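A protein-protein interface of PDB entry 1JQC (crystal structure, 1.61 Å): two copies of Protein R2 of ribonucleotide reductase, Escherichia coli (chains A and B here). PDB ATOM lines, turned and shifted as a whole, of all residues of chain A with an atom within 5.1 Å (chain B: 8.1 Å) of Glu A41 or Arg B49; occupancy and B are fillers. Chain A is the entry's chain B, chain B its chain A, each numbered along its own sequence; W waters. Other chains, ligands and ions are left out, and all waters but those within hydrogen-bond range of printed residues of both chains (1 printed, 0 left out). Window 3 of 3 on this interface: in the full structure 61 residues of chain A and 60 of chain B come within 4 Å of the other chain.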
ATOM      1  N   GLU A  37      -1.274   3.149   8.945  1.00  0.00           N
ATOM      2  CA  GLU A  37      -0.744   1.822   8.606  1.00  0.00           C
ATOM      3  C   GLU A  37      -0.671   1.743   7.053  1.00  0.00           C
ATOM      4  O   GLU A  37       0.305   1.205   6.484  1.00  0.00           O
ATOM      5  CB  GLU A  37      -1.696   0.739   9.184  1.00  0.00           C
ATOM      6  CG  GLU A  37      -1.415  -0.715   8.689  1.00  0.00           C
ATOM      7  CD  GLU A  37       0.026  -1.192   8.876  1.00  0.00           C
ATOM      8  OE1 GLU A  37       0.737  -0.740   9.802  1.00  0.00           O
ATOM      9  OE2 GLU A  37       0.465  -2.067   8.063  1.00  0.00           O
ATOM     10  N   LYS A  38      -1.680   2.272   6.346  1.00  0.00           N
ATOM     11  CA  LYS A  38      -1.637   2.263   4.889  1.00  0.00           C
ATOM     12  C   LYS A  38      -0.442   3.067   4.366  1.00  0.00           C
ATOM     13  O   LYS A  38       0.187   2.678   3.376  1.00  0.00           O
ATOM     14  CB  LYS A  38      -2.943   2.812   4.294  1.00  0.00           C
ATOM     15  CG  LYS A  38      -4.155   1.840   4.482  1.00  0.00           C
ATOM     16  CD  LYS A  38      -3.961   0.830   5.596  1.00  0.00           C
ATOM     17  CE  LYS A  38      -4.906  -0.395   5.509  1.00  0.00           C
ATOM     18  NZ  LYS A  38      -4.629  -1.344   6.666  1.00  0.00           N
ATOM     19  N   LEU A  39      -0.114   4.184   5.043  1.00  0.00           N
ATOM     20  CA  LEU A  39       1.015   4.985   4.609  1.00  0.00           C
ATOM     21  C   LEU A  39       2.329   4.240   4.874  1.00  0.00           C
ATOM     22  O   LEU A  39       3.237   4.288   4.038  1.00  0.00           O
ATOM     23  CB  LEU A  39       1.024   6.359   5.333  1.00  0.00           C
ATOM     24  CG  LEU A  39      -0.094   7.304   4.826  1.00  0.00           C
ATOM     25  CD1 LEU A  39      -0.170   8.555   5.717  1.00  0.00           C
ATOM     26  CD2 LEU A  39       0.244   7.708   3.332  1.00  0.00           C
ATOM     27  N   ILE A  40       2.434   3.565   6.000  1.00  0.00           N
ATOM     28  CA  ILE A  40       3.667   2.811   6.293  1.00  0.00           C
ATOM     29  C   ILE A  40       3.841   1.774   5.173  1.00  0.00           C
ATOM     30  O   ILE A  40       4.924   1.643   4.585  1.00  0.00           O
ATOM     31  CB  ILE A  40       3.593   2.042   7.663  1.00  0.00           C
ATOM     32  CG1 ILE A  40       3.670   3.006   8.883  1.00  0.00           C
ATOM     33  CG2 ILE A  40       4.860   1.140   7.801  1.00  0.00           C
ATOM     34  CD1 ILE A  40       2.995   2.465  10.183  1.00  0.00           C
ATOM     35  N   GLU A  41       2.765   1.040   4.882  1.00  0.00           N
ATOM     36  CA  GLU A  41       2.891   0.015   3.853  1.00  0.00           C
ATOM     37  C   GLU A  41       3.295   0.582   2.511  1.00  0.00           C
ATOM     38  O   GLU A  41       4.153  -0.003   1.816  1.00  0.00           O
ATOM     39  CB  GLU A  41       1.566  -0.764   3.682  1.00  0.00           C
ATOM     40  CG  GLU A  41       1.203  -1.559   4.919  1.00  0.00           C
ATOM     41  CD  GLU A  41      -0.207  -2.161   4.848  1.00  0.00           C
ATOM     42  OE1 GLU A  41      -0.747  -2.243   3.736  1.00  0.00           O
ATOM     43  OE2 GLU A  41      -0.749  -2.551   5.920  1.00  0.00           O
ATOM     44  N   LYS A  42       2.686   1.702   2.111  1.00  0.00           N
ATOM     45  CA  LYS A  42       3.001   2.274   0.808  1.00  0.00           C
ATOM     46  C   LYS A  42       4.452   2.771   0.765  1.00  0.00           C
ATOM     47  O   LYS A  42       5.194   2.563  -0.190  1.00  0.00           O
ATOM     48  CB  LYS A  42       2.014   3.388   0.449  1.00  0.00           C
ATOM     49  CG  LYS A  42       0.989   3.036  -0.658  1.00  0.00           C
ATOM     50  CD  LYS A  42       1.604   2.577  -1.983  1.00  0.00           C
ATOM     51  CE  LYS A  42       0.602   2.404  -3.184  1.00  0.00           C
ATOM     52  NZ  LYS A  42      -0.526   1.432  -2.938  1.00  0.00           N
ATOM     53  N   GLN A  43       4.893   3.408   1.863  1.00  0.00           N
ATOM     54  CA  GLN A  43       6.237   3.934   1.866  1.00  0.00           C
ATOM     55  C   GLN A  43       7.275   2.798   1.765  1.00  0.00           C
ATOM     56  O   GLN A  43       8.312   2.920   1.073  1.00  0.00           O
ATOM     57  CB  GLN A  43       6.426   4.801   3.145  1.00  0.00           C
ATOM     58  CG  GLN A  43       7.814   5.484   3.248  1.00  0.00           C
ATOM     59  CD  GLN A  43       8.048   6.461   2.106  1.00  0.00           C
ATOM     60  OE1 GLN A  43       7.681   7.647   2.216  1.00  0.00           O
ATOM     61  NE2 GLN A  43       8.649   5.975   0.995  1.00  0.00           N
ATOM     62  N   LEU A  44       7.014   1.702   2.469  1.00  0.00           N
ATOM     63  CA  LEU A  44       7.925   0.556   2.412  1.00  0.00           C
ATOM     64  C   LEU A  44       7.921  -0.006   0.953  1.00  0.00           C
ATOM     65  O   LEU A  44       8.993  -0.375   0.409  1.00  0.00           O
ATOM     66  CB  LEU A  44       7.505  -0.524   3.414  1.00  0.00           C
ATOM     67  CG  LEU A  44       7.571  -0.176   4.921  1.00  0.00           C
ATOM     68  CD1 LEU A  44       7.047  -1.341   5.760  1.00  0.00           C
ATOM     69  CD2 LEU A  44       8.985   0.175   5.320  1.00  0.00           C
ATOM     70  N   SER A  45       6.740   0.008   0.343  1.00  0.00           N
ATOM     71  CA  SER A  45       6.664  -0.486  -1.027  1.00  0.00           C
ATOM     72  C   SER A  45       7.417   0.356  -2.024  1.00  0.00           C
ATOM     73  O   SER A  45       7.817  -0.176  -3.086  1.00  0.00           O
ATOM     74  CB  SER A  45       5.219  -0.677  -1.477  1.00  0.00           C
ATOM     75  OG  SER A  45       4.605   0.532  -1.929  1.00  0.00           O
ATOM     76  N   PHE B  46      20.247  -4.717   3.066  1.00  0.00           N
ATOM     77  CA  PHE B  46      19.490  -5.797   3.691  1.00  0.00           C
ATOM     78  C   PHE B  46      17.976  -5.588   3.770  1.00  0.00           C
ATOM     79  O   PHE B  46      17.280  -6.456   4.323  1.00  0.00           O
ATOM     80  CB  PHE B  46      19.974  -6.002   5.148  1.00  0.00           C
ATOM     81  CG  PHE B  46      21.342  -6.563   5.253  1.00  0.00           C
ATOM     82  CD1 PHE B  46      21.937  -7.198   4.162  1.00  0.00           C
ATOM     83  CD2 PHE B  46      22.043  -6.483   6.465  1.00  0.00           C
ATOM     84  CE1 PHE B  46      23.209  -7.747   4.261  1.00  0.00           C
ATOM     85  CE2 PHE B  46      23.339  -7.050   6.557  1.00  0.00           C
ATOM     86  CZ  PHE B  46      23.905  -7.673   5.451  1.00  0.00           C
ATOM     87  N   PHE B  47      17.465  -4.441   3.303  1.00  0.00           N
ATOM     88  CA  PHE B  47      16.026  -4.125   3.379  1.00  0.00           C
ATOM     89  C   PHE B  47      15.142  -5.335   3.054  1.00  0.00           C
ATOM     90  O   PHE B  47      15.331  -5.972   2.001  1.00  0.00           O
ATOM     91  CB  PHE B  47      15.723  -2.988   2.385  1.00  0.00           C
ATOM     92  CG  PHE B  47      14.345  -2.406   2.505  1.00  0.00           C
ATOM     93  CD1 PHE B  47      14.105  -1.329   3.368  1.00  0.00           C
ATOM     94  CD2 PHE B  47      13.294  -2.929   1.750  1.00  0.00           C
ATOM     95  CE1 PHE B  47      12.787  -0.767   3.483  1.00  0.00           C
ATOM     96  CE2 PHE B  47      11.992  -2.407   1.844  1.00  0.00           C
ATOM     97  CZ  PHE B  47      11.731  -1.328   2.709  1.00  0.00           C
ATOM     98  N   TRP B  48      14.202  -5.641   3.946  1.00  0.00           N
ATOM     99  CA  TRP B  48      13.289  -6.763   3.730  1.00  0.00           C
ATOM    100  C   TRP B  48      11.912  -6.390   4.221  1.00  0.00           C
ATOM    101  O   TRP B  48      11.760  -5.519   5.071  1.00  0.00           O
ATOM    102  CB  TRP B  48      13.810  -8.045   4.401  1.00  0.00           C
ATOM    103  CG  TRP B  48      14.075  -7.965   5.887  1.00  0.00           C
ATOM    104  CD1 TRP B  48      15.197  -7.437   6.494  1.00  0.00           C
ATOM    105  CD2 TRP B  48      13.259  -8.470   6.935  1.00  0.00           C
ATOM    106  NE1 TRP B  48      15.124  -7.599   7.855  1.00  0.00           N
ATOM    107  CE2 TRP B  48      13.946  -8.216   8.165  1.00  0.00           C
ATOM    108  CE3 TRP B  48      12.023  -9.117   6.972  1.00  0.00           C
ATOM    109  CZ2 TRP B  48      13.427  -8.583   9.395  1.00  0.00           C
ATOM    110  CZ3 TRP B  48      11.500  -9.485   8.216  1.00  0.00           C
ATOM    111  CH2 TRP B  48      12.203  -9.216   9.422  1.00  0.00           C
ATOM    112  N   ARG B  49      10.881  -7.023   3.647  1.00  0.00           N
ATOM    113  CA  ARG B  49       9.492  -6.730   4.016  1.00  0.00           C
ATOM    114  C   ARG B  49       8.943  -7.974   4.674  1.00  0.00           C
ATOM    115  O   ARG B  49       8.794  -9.005   4.038  1.00  0.00           O
ATOM    116  CB  ARG B  49       8.699  -6.382   2.737  1.00  0.00           C
ATOM    117  CG  ARG B  49       7.210  -6.026   2.947  1.00  0.00           C
ATOM    118  CD  ARG B  49       6.989  -4.623   3.581  1.00  0.00           C
ATOM    119  NE  ARG B  49       5.553  -4.388   3.807  1.00  0.00           N
ATOM    120  CZ  ARG B  49       4.762  -3.715   2.965  1.00  0.00           C
ATOM    121  NH1 ARG B  49       5.250  -3.179   1.857  1.00  0.00           N
ATOM    122  NH2 ARG B  49       3.458  -3.650   3.191  1.00  0.00           N
ATOM    123  N   PRO B  50       8.611  -7.893   5.960  1.00  0.00           N
ATOM    124  CA  PRO B  50       8.090  -9.041   6.698  1.00  0.00           C
ATOM    125  C   PRO B  50       6.876  -9.763   6.115  1.00  0.00           C
ATOM    126  O   PRO B  50       6.809 -11.002   6.116  1.00  0.00           O
ATOM    127  CB  PRO B  50       7.762  -8.439   8.059  1.00  0.00           C
ATOM    128  CG  PRO B  50       8.720  -7.253   8.166  1.00  0.00           C
ATOM    129  CD  PRO B  50       8.629  -6.683   6.795  1.00  0.00           C
ATOM    130  N   GLU B  51       5.928  -8.969   5.644  1.00  0.00           N
ATOM    131  CA  GLU B  51       4.686  -9.534   5.148  1.00  0.00           C
ATOM    132  C   GLU B  51       4.858 -10.486   3.996  1.00  0.00           C
ATOM    133  O   GLU B  51       3.980 -11.317   3.766  1.00  0.00           O
ATOM    134  CB  GLU B  51       3.729  -8.429   4.735  1.00  0.00           C
ATOM    135  CG  GLU B  51       3.181  -7.572   5.863  1.00  0.00           C
ATOM    136  CD  GLU B  51       4.151  -6.503   6.365  1.00  0.00           C
ATOM    137  OE1 GLU B  51       5.220  -6.236   5.735  1.00  0.00           O
ATOM    138  OE2 GLU B  51       3.821  -5.921   7.420  1.00  0.00           O
ATOM    139  N   GLU B  52       5.952 -10.344   3.260  1.00  0.00           N
ATOM    140  CA  GLU B  52       6.218 -11.208   2.130  1.00  0.00           C
ATOM    141  C   GLU B  52       6.678 -12.586   2.572  1.00  0.00           C
ATOM    142  O   GLU B  52       6.657 -13.526   1.782  1.00  0.00           O
ATOM    143  CB  GLU B  52       7.300 -10.603   1.231  1.00  0.00           C
ATOM    144  CG  GLU B  52       6.837  -9.385   0.424  1.00  0.00           C
ATOM    145  CD  GLU B  52       7.985  -8.673  -0.265  1.00  0.00           C
ATOM    146  OE1 GLU B  52       9.084  -9.264  -0.384  1.00  0.00           O
ATOM    147  OE2 GLU B  52       7.779  -7.518  -0.708  1.00  0.00           O
ATOM    148  N   VAL B  53       7.112 -12.719   3.823  1.00  0.00           N
ATOM    149  CA  VAL B  53       7.556 -14.029   4.254  1.00  0.00           C
ATOM    150  C   VAL B  53       6.359 -14.930   4.492  1.00  0.00           C
ATOM    151  O   VAL B  53       5.413 -14.606   5.221  1.00  0.00           O
ATOM    152  CB  VAL B  53       8.440 -13.973   5.553  1.00  0.00           C
ATOM    153  CG1 VAL B  53       8.837 -15.385   5.961  1.00  0.00           C
ATOM    154  CG2 VAL B  53       9.711 -13.182   5.288  1.00  0.00           C
ATOM    155  N   ASP B  54       6.408 -16.097   3.871  1.00  0.00           N
ATOM    156  CA  ASP B  54       5.325 -17.055   4.007  1.00  0.00           C
ATOM    157  C   ASP B  54       5.297 -17.689   5.411  1.00  0.00           C
ATOM    158  O   ASP B  54       6.176 -18.469   5.750  1.00  0.00           O
ATOM    159  CB  ASP B  54       5.515 -18.140   2.937  1.00  0.00           C
ATOM    160  CG  ASP B  54       4.394 -19.148   2.906  1.00  0.00           C
ATOM    161  OD1 ASP B  54       3.410 -19.022   3.677  1.00  0.00           O
ATOM    162  OD2 ASP B  54       4.522 -20.089   2.087  1.00  0.00           O
ATOM    163  N   ILE B 117      10.835  -2.498  11.557  1.00  0.00           N
ATOM    164  CA  ILE B 117      10.554  -3.605  10.642  1.00  0.00           C
ATOM    165  C   ILE B 117      10.528  -4.899  11.455  1.00  0.00           C
ATOM    166  O   ILE B 117       9.663  -5.798  11.240  1.00  0.00           O
ATOM    167  CB  ILE B 117      11.603  -3.658   9.526  1.00  0.00           C
ATOM    168  CG1 ILE B 117      11.471  -2.391   8.635  1.00  0.00           C
ATOM    169  CG2 ILE B 117      11.413  -4.984   8.686  1.00  0.00           C
ATOM    170  CD1 ILE B 117      10.138  -2.283   7.837  1.00  0.00           C
ATOM    171  N   ARG B 120       7.227  -5.125  13.085  1.00  0.00           N
ATOM    172  CA  ARG B 120       6.189  -5.436  12.084  1.00  0.00           C
ATOM    173  C   ARG B 120       6.230  -6.951  11.798  1.00  0.00           C
ATOM    174  O   ARG B 120       5.169  -7.570  11.623  1.00  0.00           O
ATOM    175  CB  ARG B 120       6.480  -4.627  10.828  1.00  0.00           C
ATOM    176  CG  ARG B 120       6.178  -3.165  11.095  1.00  0.00           C
ATOM    177  CD  ARG B 120       6.253  -2.269   9.839  1.00  0.00           C
ATOM    178  NE  ARG B 120       5.245  -2.695   8.877  1.00  0.00           N
ATOM    179  CZ  ARG B 120       3.955  -2.356   8.875  1.00  0.00           C
ATOM    180  NH1 ARG B 120       3.448  -1.524   9.768  1.00  0.00           N
ATOM    181  NH2 ARG B 120       3.152  -2.940   8.004  1.00  0.00           N
ATOM    182  N   SER B 121       7.437  -7.522  11.789  1.00  0.00           N
ATOM    183  CA  SER B 121       7.535  -8.990  11.510  1.00  0.00           C
ATOM    184  C   SER B 121       6.891  -9.780  12.653  1.00  0.00           C
ATOM    185  O   SER B 121       6.274 -10.835  12.400  1.00  0.00           O
ATOM    186  CB  SER B 121       9.003  -9.401  11.293  1.00  0.00           C
ATOM    187  OG  SER B 121       9.754  -9.546  12.479  1.00  0.00           O
ATOM    188  N   HIS B 124       3.279  -9.907  12.082  1.00  0.00           N
ATOM    189  CA  HIS B 124       2.986 -10.831  10.995  1.00  0.00           C
ATOM    190  C   HIS B 124       3.003 -12.268  11.517  1.00  0.00           C
ATOM    191  O   HIS B 124       2.133 -13.093  11.150  1.00  0.00           O
ATOM    192  CB  HIS B 124       4.025 -10.606   9.904  1.00  0.00           C
ATOM    193  CG  HIS B 124       3.862 -11.482   8.705  1.00  0.00           C
ATOM    194  ND1 HIS B 124       2.706 -11.532   7.951  1.00  0.00           N
ATOM    195  CD2 HIS B 124       4.738 -12.317   8.117  1.00  0.00           C
ATOM    196  CE1 HIS B 124       2.892 -12.359   6.935  1.00  0.00           C
ATOM    197  NE2 HIS B 124       4.113 -12.846   7.014  1.00  0.00           N
ATOM    198  N   ILE B 230      12.291 -15.338   9.304  1.00  0.00           N
ATOM    199  CA  ILE B 230      12.231 -13.973   9.839  1.00  0.00           C
ATOM    200  C   ILE B 230      13.328 -13.757  10.872  1.00  0.00           C
ATOM    201  O   ILE B 230      14.062 -12.739  10.803  1.00  0.00           O
ATOM    202  CB  ILE B 230      10.836 -13.707  10.459  1.00  0.00           C
ATOM    203  CG1 ILE B 230       9.827 -13.552   9.293  1.00  0.00           C
ATOM    204  CG2 ILE B 230      10.876 -12.496  11.416  1.00  0.00           C
ATOM    205  CD1 ILE B 230       8.342 -13.476   9.761  1.00  0.00           C
ATOM    206  N   LEU B 233      16.572 -13.172   9.247  1.00  0.00           N
ATOM    207  CA  LEU B 233      16.745 -11.833   8.698  1.00  0.00           C
ATOM    208  C   LEU B 233      16.998 -10.845   9.837  1.00  0.00           C
ATOM    209  O   LEU B 233      17.822  -9.929   9.692  1.00  0.00           O
ATOM    210  CB  LEU B 233      15.466 -11.423   7.954  1.00  0.00           C
ATOM    211  CG  LEU B 233      15.409 -12.210   6.631  1.00  0.00           C
ATOM    212  CD1 LEU B 233      13.962 -12.138   6.143  1.00  0.00           C
ATOM    213  CD2 LEU B 233      16.396 -11.671   5.588  1.00  0.00           C
HETATM  214  O   HOH W   1       8.294  -3.263   0.700  1.00  0.00           O
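The backbone carbonyl oxygen (O) of Glu A41 sits at hydrogen-bond distance from the guanidinium group (NH1) of Arg B49. OE1 of Glu A37 is in salt-bridge range of NH1 of Arg B120 (2.8 Å).
The guanidinium group (NE) of Arg B49 is in salt-bridge range of the side-chain carboxylate (OE1) of Glu B51, at 2.7 Å. The backbone carbonyl oxygen (O) of Lys A42 sits at hydrogen-bond distance from the side-chain hydroxyl (OG) of Ser A45 (2.7 Å). The side-chain carboxylate (OE2) of Glu B51 lies within salt-bridge range of the guanidinium group (NH2) of Arg B120, 3.1 Å away. The side-chain carboxylate (OE2) of Glu A37 sits close to the side-chain carboxylate (OE2) of Glu A41 (2.5 Å).
Arg B120 touches Ile A40. Arg B120 touches Glu A41 (NH2 to CG, 3.9 Å). O of Leu A44 touches CZ of Phe B47, 3.7 Å away. Arg B49 touches Leu A44. Leu A44 touches Ile B117. CD1 of Leu A44 touches NE of Arg B120, at 3.8 Å. N of Ser A45 touches NH1 of Arg B49, at 3.8 Å.
Of chain B, only Arg B49 and Arg B120 come within 4 Å of Glu A41. Of chain A, only Glu A41 (3.4 Å), Leu A44 (3.8 Å) and Ser A45 (3.8 Å) come within 4 Å of Arg B49. Of the printed residues of chain A, Ile B117 touches Leu A44. Printed residues of chain A within 4 Å of Arg B120: Glu A37, Ile A40, Glu A41 and Leu A44. Of the printed residues of chain A, Phe B47 touches Leu A44 (3.7 Å). Of the printed residues of chain B, Leu A44 touches Phe B47 (3.7 Å), Arg B49 (3.8 Å), Ile B117 (3.7 Å) and Arg B120 (3.8 Å). Of the printed residues of chain B, Ser A45 touches Arg B49 (3.8 Å). Lys A38 touches none of the printed residues of chain B. The nearest residue of chain B that does not touch Glu A41 is Glu B51 (5.7 Å). The nearest printed residue of chain A that does not touch Arg B49 is Lys A42 (5.5 Å). The nearest printed residue of chain B that does not touch Ser A45 is Phe B47 (5.7 Å).
Among the printed residues, 9 pairs touch across the chains. Among the printed residues, Asp or Glu carboxylates within 4 Å of a Lys or Arg side-chain nitrogen of the other chain: Glu A37 with Arg B120 (2.8 Å).
No position is printed for both chains. Of the 9 pairs that touch across the chains among the printed residues, none has its exchanged pair printed and touching as well.
Water W1 lies within hydrogen-bond range of O of Leu A44 (3.0 Å) and NH1 of Arg B49 (3.3 Å).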
